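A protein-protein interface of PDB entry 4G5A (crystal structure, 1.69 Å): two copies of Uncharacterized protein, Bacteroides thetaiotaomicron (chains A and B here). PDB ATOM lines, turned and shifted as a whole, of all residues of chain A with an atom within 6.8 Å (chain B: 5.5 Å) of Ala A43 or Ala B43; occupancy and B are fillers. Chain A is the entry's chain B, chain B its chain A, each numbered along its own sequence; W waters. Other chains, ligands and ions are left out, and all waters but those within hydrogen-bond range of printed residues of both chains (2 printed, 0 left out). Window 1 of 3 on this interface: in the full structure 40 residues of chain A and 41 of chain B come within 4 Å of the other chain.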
ATOM      1  N   PHE A  38     -15.704 -26.996  36.911  1.00  0.00           N
ATOM      2  CA  PHE A  38     -14.561 -26.116  37.009  1.00  0.00           C
ATOM      3  C   PHE A  38     -14.473 -25.528  38.415  1.00  0.00           C
ATOM      4  O   PHE A  38     -15.439 -24.944  38.898  1.00  0.00           O
ATOM      5  CB  PHE A  38     -14.710 -24.986  35.979  1.00  0.00           C
ATOM      6  CG  PHE A  38     -14.638 -25.450  34.560  1.00  0.00           C
ATOM      7  CD1 PHE A  38     -15.764 -25.919  33.907  1.00  0.00           C
ATOM      8  CD2 PHE A  38     -13.432 -25.397  33.854  1.00  0.00           C
ATOM      9  CE1 PHE A  38     -15.692 -26.320  32.586  1.00  0.00           C
ATOM     10  CE2 PHE A  38     -13.353 -25.815  32.548  1.00  0.00           C
ATOM     11  CZ  PHE A  38     -14.481 -26.291  31.913  1.00  0.00           C
ATOM     12  N   SER A  41     -13.307 -20.008  37.206  1.00  0.00           N
ATOM     13  CA  SER A  41     -13.648 -19.662  35.844  1.00  0.00           C
ATOM     14  C   SER A  41     -12.447 -19.894  34.910  1.00  0.00           C
ATOM     15  O   SER A  41     -11.320 -20.086  35.368  1.00  0.00           O
ATOM     16  CB  SER A  41     -14.158 -18.237  35.739  1.00  0.00           C
ATOM     17  OG  SER A  41     -13.252 -17.337  36.298  1.00  0.00           O
ATOM     18  N   PHE A  42     -12.723 -19.883  33.610  1.00  0.00           N
ATOM     19  CA  PHE A  42     -11.753 -20.307  32.577  1.00  0.00           C
ATOM     20  C   PHE A  42     -12.118 -19.711  31.235  1.00  0.00           C
ATOM     21  O   PHE A  42     -13.239 -19.234  31.033  1.00  0.00           O
ATOM     22  CB  PHE A  42     -11.713 -21.844  32.489  1.00  0.00           C
ATOM     23  CG  PHE A  42     -10.447 -22.408  31.875  1.00  0.00           C
ATOM     24  CD1 PHE A  42      -9.227 -22.258  32.528  1.00  0.00           C
ATOM     25  CD2 PHE A  42     -10.485 -23.120  30.680  1.00  0.00           C
ATOM     26  CE1 PHE A  42      -8.059 -22.789  31.995  1.00  0.00           C
ATOM     27  CE2 PHE A  42      -9.327 -23.667  30.143  1.00  0.00           C
ATOM     28  CZ  PHE A  42      -8.108 -23.486  30.789  1.00  0.00           C
ATOM     29  N   ALA A  43     -11.142 -19.690  30.324  1.00  0.00           N
ATOM     30  CA  ALA A  43     -11.370 -19.252  28.953  1.00  0.00           C
ATOM     31  C   ALA A  43     -12.338 -20.218  28.251  1.00  0.00           C
ATOM     32  O   ALA A  43     -12.439 -21.397  28.640  1.00  0.00           O
ATOM     33  CB  ALA A  43     -10.019 -19.215  28.188  1.00  0.00           C
ATOM     34  N   PRO A  44     -13.010 -19.743  27.186  1.00  0.00           N
ATOM     35  CA  PRO A  44     -13.820 -20.662  26.389  1.00  0.00           C
ATOM     36  C   PRO A  44     -12.987 -21.885  25.935  1.00  0.00           C
ATOM     37  O   PRO A  44     -11.786 -21.764  25.631  1.00  0.00           O
ATOM     38  CB  PRO A  44     -14.235 -19.811  25.193  1.00  0.00           C
ATOM     39  CG  PRO A  44     -14.310 -18.435  25.735  1.00  0.00           C
ATOM     40  CD  PRO A  44     -13.128 -18.349  26.699  1.00  0.00           C
ATOM     41  N   ILE A  45     -13.635 -23.040  25.887  1.00  0.00           N
ATOM     42  CA  ILE A  45     -12.933 -24.283  25.589  1.00  0.00           C
ATOM     43  C   ILE A  45     -13.780 -25.138  24.667  1.00  0.00           C
ATOM     44  O   ILE A  45     -14.996 -25.269  24.859  1.00  0.00           O
ATOM     45  CB  ILE A  45     -12.556 -25.025  26.907  1.00  0.00           C
ATOM     46  CG1 ILE A  45     -11.658 -26.232  26.621  1.00  0.00           C
ATOM     47  CG2 ILE A  45     -13.797 -25.403  27.753  1.00  0.00           C
ATOM     48  CD1 ILE A  45     -10.930 -26.741  27.907  1.00  0.00           C
ATOM     49  N   THR A  46     -13.113 -25.674  23.649  1.00  0.00           N
ATOM     50  CA  THR A  46     -13.783 -26.524  22.663  1.00  0.00           C
ATOM     51  C   THR A  46     -13.819 -27.946  23.226  1.00  0.00           C
ATOM     52  O   THR A  46     -12.803 -28.435  23.733  1.00  0.00           O
ATOM     53  CB  THR A  46     -13.061 -26.496  21.283  1.00  0.00           C
ATOM     54  OG1 THR A  46     -13.110 -25.170  20.713  1.00  0.00           O
ATOM     55  CG2 THR A  46     -13.717 -27.520  20.285  1.00  0.00           C
ATOM     56  N   ILE A  62     -17.706 -24.427  25.195  1.00  0.00           N
ATOM     57  CA  ILE A  62     -18.211 -24.145  26.522  1.00  0.00           C
ATOM     58  C   ILE A  62     -17.599 -22.818  26.973  1.00  0.00           C
ATOM     59  O   ILE A  62     -16.438 -22.552  26.660  1.00  0.00           O
ATOM     60  CB  ILE A  62     -17.823 -25.295  27.498  1.00  0.00           C
ATOM     61  CG1 ILE A  62     -18.528 -26.585  27.074  1.00  0.00           C
ATOM     62  CG2 ILE A  62     -18.181 -24.974  28.929  1.00  0.00           C
ATOM     63  CD1 ILE A  62     -20.014 -26.405  26.990  1.00  0.00           C
ATOM     64  N   PHE A  63     -18.378 -21.997  27.687  1.00  0.00           N
ATOM     65  CA  PHE A  63     -17.926 -20.685  28.211  1.00  0.00           C
ATOM     66  C   PHE A  63     -17.959 -20.666  29.739  1.00  0.00           C
ATOM     67  O   PHE A  63     -18.964 -20.255  30.346  1.00  0.00           O
ATOM     68  CB  PHE A  63     -18.818 -19.575  27.629  1.00  0.00           C
ATOM     69  CG  PHE A  63     -18.795 -19.517  26.126  1.00  0.00           C
ATOM     70  CD1 PHE A  63     -19.636 -20.325  25.360  1.00  0.00           C
ATOM     71  CD2 PHE A  63     -17.910 -18.700  25.472  1.00  0.00           C
ATOM     72  CE1 PHE A  63     -19.595 -20.285  23.959  1.00  0.00           C
ATOM     73  CE2 PHE A  63     -17.852 -18.654  24.081  1.00  0.00           C
ATOM     74  CZ  PHE A  63     -18.700 -19.448  23.330  1.00  0.00           C
ATOM     75  N   PRO A  64     -16.869 -21.103  30.381  1.00  0.00           N
ATOM     76  CA  PRO A  64     -16.871 -21.233  31.845  1.00  0.00           C
ATOM     77  C   PRO A  64     -16.665 -19.901  32.579  1.00  0.00           C
ATOM     78  O   PRO A  64     -15.626 -19.641  33.201  1.00  0.00           O
ATOM     79  CB  PRO A  64     -15.782 -22.281  32.122  1.00  0.00           C
ATOM     80  CG  PRO A  64     -15.336 -22.773  30.755  1.00  0.00           C
ATOM     81  CD  PRO A  64     -15.667 -21.723  29.781  1.00  0.00           C
ATOM     82  N   ASN A  88      -8.064 -25.343  24.254  1.00  0.00           N
ATOM     83  CA  ASN A  88      -8.007 -23.948  23.816  1.00  0.00           C
ATOM     84  C   ASN A  88      -6.539 -23.597  23.749  1.00  0.00           C
ATOM     85  O   ASN A  88      -5.704 -24.501  23.799  1.00  0.00           O
ATOM     86  CB  ASN A  88      -8.827 -23.005  24.704  1.00  0.00           C
ATOM     87  CG  ASN A  88      -8.430 -23.036  26.167  1.00  0.00           C
ATOM     88  OD1 ASN A  88      -7.320 -23.455  26.527  1.00  0.00           O
ATOM     89  ND2 ASN A  88      -9.366 -22.605  27.036  1.00  0.00           N
ATOM     90  N   ALA A  89      -6.218 -22.303  23.655  1.00  0.00           N
ATOM     91  CA  ALA A  89      -4.827 -21.889  23.479  1.00  0.00           C
ATOM     92  C   ALA A  89      -3.906 -22.333  24.593  1.00  0.00           C
ATOM     93  O   ALA A  89      -2.689 -22.483  24.342  1.00  0.00           O
ATOM     94  CB  ALA A  89      -4.729 -20.344  23.349  1.00  0.00           C
ATOM     95  N   SER A  90      -4.487 -22.538  25.773  1.00  0.00           N
ATOM     96  CA  SER A  90      -3.750 -22.782  27.017  1.00  0.00           C
ATOM     97  C   SER A  90      -3.642 -24.237  27.492  1.00  0.00           C
ATOM     98  O   SER A  90      -2.698 -24.576  28.198  1.00  0.00           O
ATOM     99  CB  SER A  90      -4.369 -21.982  28.156  1.00  0.00           C
ATOM    100  OG  SER A  90      -5.350 -22.715  28.859  1.00  0.00           O
ATOM    101  N   SER B  41     -10.043 -15.215  22.796  1.00  0.00           N
ATOM    102  CA  SER B  41     -10.859 -15.238  24.002  1.00  0.00           C
ATOM    103  C   SER B  41      -9.953 -15.576  25.199  1.00  0.00           C
ATOM    104  O   SER B  41      -8.797 -16.009  25.018  1.00  0.00           O
ATOM    105  CB  SER B  41     -12.008 -16.231  23.877  1.00  0.00           C
ATOM    106  OG  SER B  41     -11.552 -17.498  23.447  1.00  0.00           O
ATOM    107  N   PHE B  42     -10.488 -15.377  26.397  1.00  0.00           N
ATOM    108  CA  PHE B  42      -9.720 -15.426  27.645  1.00  0.00           C
ATOM    109  C   PHE B  42     -10.665 -15.675  28.815  1.00  0.00           C
ATOM    110  O   PHE B  42     -11.875 -15.481  28.709  1.00  0.00           O
ATOM    111  CB  PHE B  42      -8.936 -14.116  27.808  1.00  0.00           C
ATOM    112  CG  PHE B  42      -7.745 -14.215  28.714  1.00  0.00           C
ATOM    113  CD1 PHE B  42      -6.667 -15.011  28.372  1.00  0.00           C
ATOM    114  CD2 PHE B  42      -7.696 -13.509  29.921  1.00  0.00           C
ATOM    115  CE1 PHE B  42      -5.543 -15.091  29.199  1.00  0.00           C
ATOM    116  CE2 PHE B  42      -6.591 -13.603  30.765  1.00  0.00           C
ATOM    117  CZ  PHE B  42      -5.513 -14.395  30.408  1.00  0.00           C
ATOM    118  N   ALA B  43     -10.100 -16.134  29.921  1.00  0.00           N
ATOM    119  CA  ALA B  43     -10.818 -16.288  31.158  1.00  0.00           C
ATOM    120  C   ALA B  43     -11.277 -14.923  31.668  1.00  0.00           C
ATOM    121  O   ALA B  43     -10.641 -13.905  31.364  1.00  0.00           O
ATOM    122  CB  ALA B  43      -9.931 -16.959  32.211  1.00  0.00           C
ATOM    123  N   PRO B  44     -12.328 -14.908  32.505  1.00  0.00           N
ATOM    124  CA  PRO B  44     -12.714 -13.665  33.172  1.00  0.00           C
ATOM    125  C   PRO B  44     -11.540 -13.052  33.911  1.00  0.00           C
ATOM    126  O   PRO B  44     -10.715 -13.756  34.501  1.00  0.00           O
ATOM    127  CB  PRO B  44     -13.804 -14.097  34.164  1.00  0.00           C
ATOM    128  CG  PRO B  44     -14.394 -15.331  33.517  1.00  0.00           C
ATOM    129  CD  PRO B  44     -13.218 -16.029  32.855  1.00  0.00           C
ATOM    130  N   ILE B  45     -11.485 -11.730  33.868  1.00  0.00           N
ATOM    131  CA  ILE B  45     -10.391 -11.008  34.477  1.00  0.00           C
ATOM    132  C   ILE B  45     -10.907  -9.796  35.250  1.00  0.00           C
ATOM    133  O   ILE B  45     -11.796  -9.095  34.776  1.00  0.00           O
ATOM    134  CB  ILE B  45      -9.319 -10.629  33.402  1.00  0.00           C
ATOM    135  CG1 ILE B  45      -8.063 -10.059  34.036  1.00  0.00           C
ATOM    136  CG2 ILE B  45      -9.868  -9.710  32.361  1.00  0.00           C
ATOM    137  CD1 ILE B  45      -6.854 -10.068  33.105  1.00  0.00           C
ATOM    138  N   ILE B  62     -14.392  -8.413  33.590  1.00  0.00           N
ATOM    139  CA  ILE B  62     -14.645  -8.489  32.159  1.00  0.00           C
ATOM    140  C   ILE B  62     -14.643  -9.969  31.768  1.00  0.00           C
ATOM    141  O   ILE B  62     -13.860 -10.727  32.307  1.00  0.00           O
ATOM    142  CB  ILE B  62     -13.524  -7.760  31.389  1.00  0.00           C
ATOM    143  CG1 ILE B  62     -13.475  -6.279  31.818  1.00  0.00           C
ATOM    144  CG2 ILE B  62     -13.678  -7.886  29.868  1.00  0.00           C
ATOM    145  CD1 ILE B  62     -14.844  -5.610  31.890  1.00  0.00           C
ATOM    146  N   PRO B  64     -14.071 -12.004  28.543  1.00  0.00           N
ATOM    147  CA  PRO B  64     -13.667 -11.966  27.144  1.00  0.00           C
ATOM    148  C   PRO B  64     -14.007 -13.278  26.414  1.00  0.00           C
ATOM    149  O   PRO B  64     -13.115 -14.033  26.011  1.00  0.00           O
ATOM    150  CB  PRO B  64     -12.150 -11.677  27.199  1.00  0.00           C
ATOM    151  CG  PRO B  64     -11.842 -11.399  28.636  1.00  0.00           C
ATOM    152  CD  PRO B  64     -12.902 -12.074  29.432  1.00  0.00           C
ATOM    153  N   ASN B  88      -6.155 -12.396  37.000  1.00  0.00           N
ATOM    154  CA  ASN B  88      -6.874 -13.644  37.303  1.00  0.00           C
ATOM    155  C   ASN B  88      -5.855 -14.694  37.689  1.00  0.00           C
ATOM    156  O   ASN B  88      -4.680 -14.369  37.865  1.00  0.00           O
ATOM    157  CB  ASN B  88      -7.834 -14.062  36.194  1.00  0.00           C
ATOM    158  CG  ASN B  88      -7.170 -14.356  34.875  1.00  0.00           C
ATOM    159  OD1 ASN B  88      -5.978 -14.649  34.812  1.00  0.00           O
ATOM    160  ND2 ASN B  88      -7.959 -14.251  33.786  1.00  0.00           N
HETATM  161  O   HOH W   1     -10.295 -19.601  24.584  1.00  0.00           O
HETATM  162  O   HOH W   2     -10.784 -16.315  35.565  1.00  0.00           O
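Ser A41 touches Pro B44, and with the chains exchanged Pro A44 touches Ser B41.
Phe A42 touches Ala B43, and with the chains exchanged Ala A43 touches Phe B42.
Phe A42 touches Pro B44, and with the chains exchanged Pro A44 touches Phe B42.
Ala A43 touches its own counterpart, Ala B43.
8 positions are printed for both chains.
N of Phe B42 lies within hydrogen-bond range of O of Pro B64 (3.0 Å).
The backbone carbonyl oxygen of Pro B44 lies within hydrogen-bond range of the side-chain amide nitrogen of Asn B88, at 2.9 Å.
The backbone carbonyl oxygen (O) of Pro A64 sits at hydrogen-bond distance from the backbone NH (N) of Phe A42 (2.9 Å).
The backbone carbonyl oxygen of Pro A44 lies within hydrogen-bond range of the side-chain amide nitrogen of Asn A88.
Printed residues of chain B that touch a printed residue of chain A: Ser B41, Phe B42, Ala B43 and Pro B44.
Hydrophobic or aromatic side chains of chain B within 4 Å of the printed part of chain A: Ala B43 and Pro B44.
Along chain B the printed residues that touch a printed residue of chain A span positions 41 to 44.
Among the printed residues, 7 pairs touch across the chains.
Water W1 lies within hydrogen-bond range of OG of Ser B41 (2.7 Å) and O of Pro A44 (2.8 Å).
Water W2 lies within hydrogen-bond range of OG of Ser A41 (2.8 Å) and O of Pro B44 (2.8 Å).
Printed residues of chain B within 4 Å of Ala A43: Phe B42 and Ala B43.
Ala B43 touches just these residues of chain A: Phe A42 (3.6 Å) and Ala A43 (3.5 Å).
Printed residues of chain B within 4 Å of Ser A41: Pro B44 (3.6 Å).
Printed residues of chain A within 4 Å of Pro B44: Ser A41 and Phe A42.
Of the printed residues of chain A, Phe B42 touches Ala A43 (3.6 Å) and Pro A44 (3.7 Å).
Printed residues of chain A within 4 Å of Ser B41: Pro A44 (3.7 Å).
Of the printed residues of chain B, Pro A44 touches Ser B41 and Phe B42.
Asn A88 touches none of the printed residues of chain B.
Ile A62 touches none of the printed residues of chain B.
The nearest printed residue of chain B that does not touch Pro A44 is Pro B64 (4.4 Å).
Ser A41 touches Pro B44 (OG to CG, 3.6 Å).
Ala B43 touches Phe A42.
Phe A42 touches Pro B44.
Ala A43 touches Phe B42.
Ala A43 touches Ala B43 (CA to N, 3.5 Å).
Pro A44 touches Ser B41 (CG to CB, 3.7 Å).
Phe B42 touches Pro A44.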
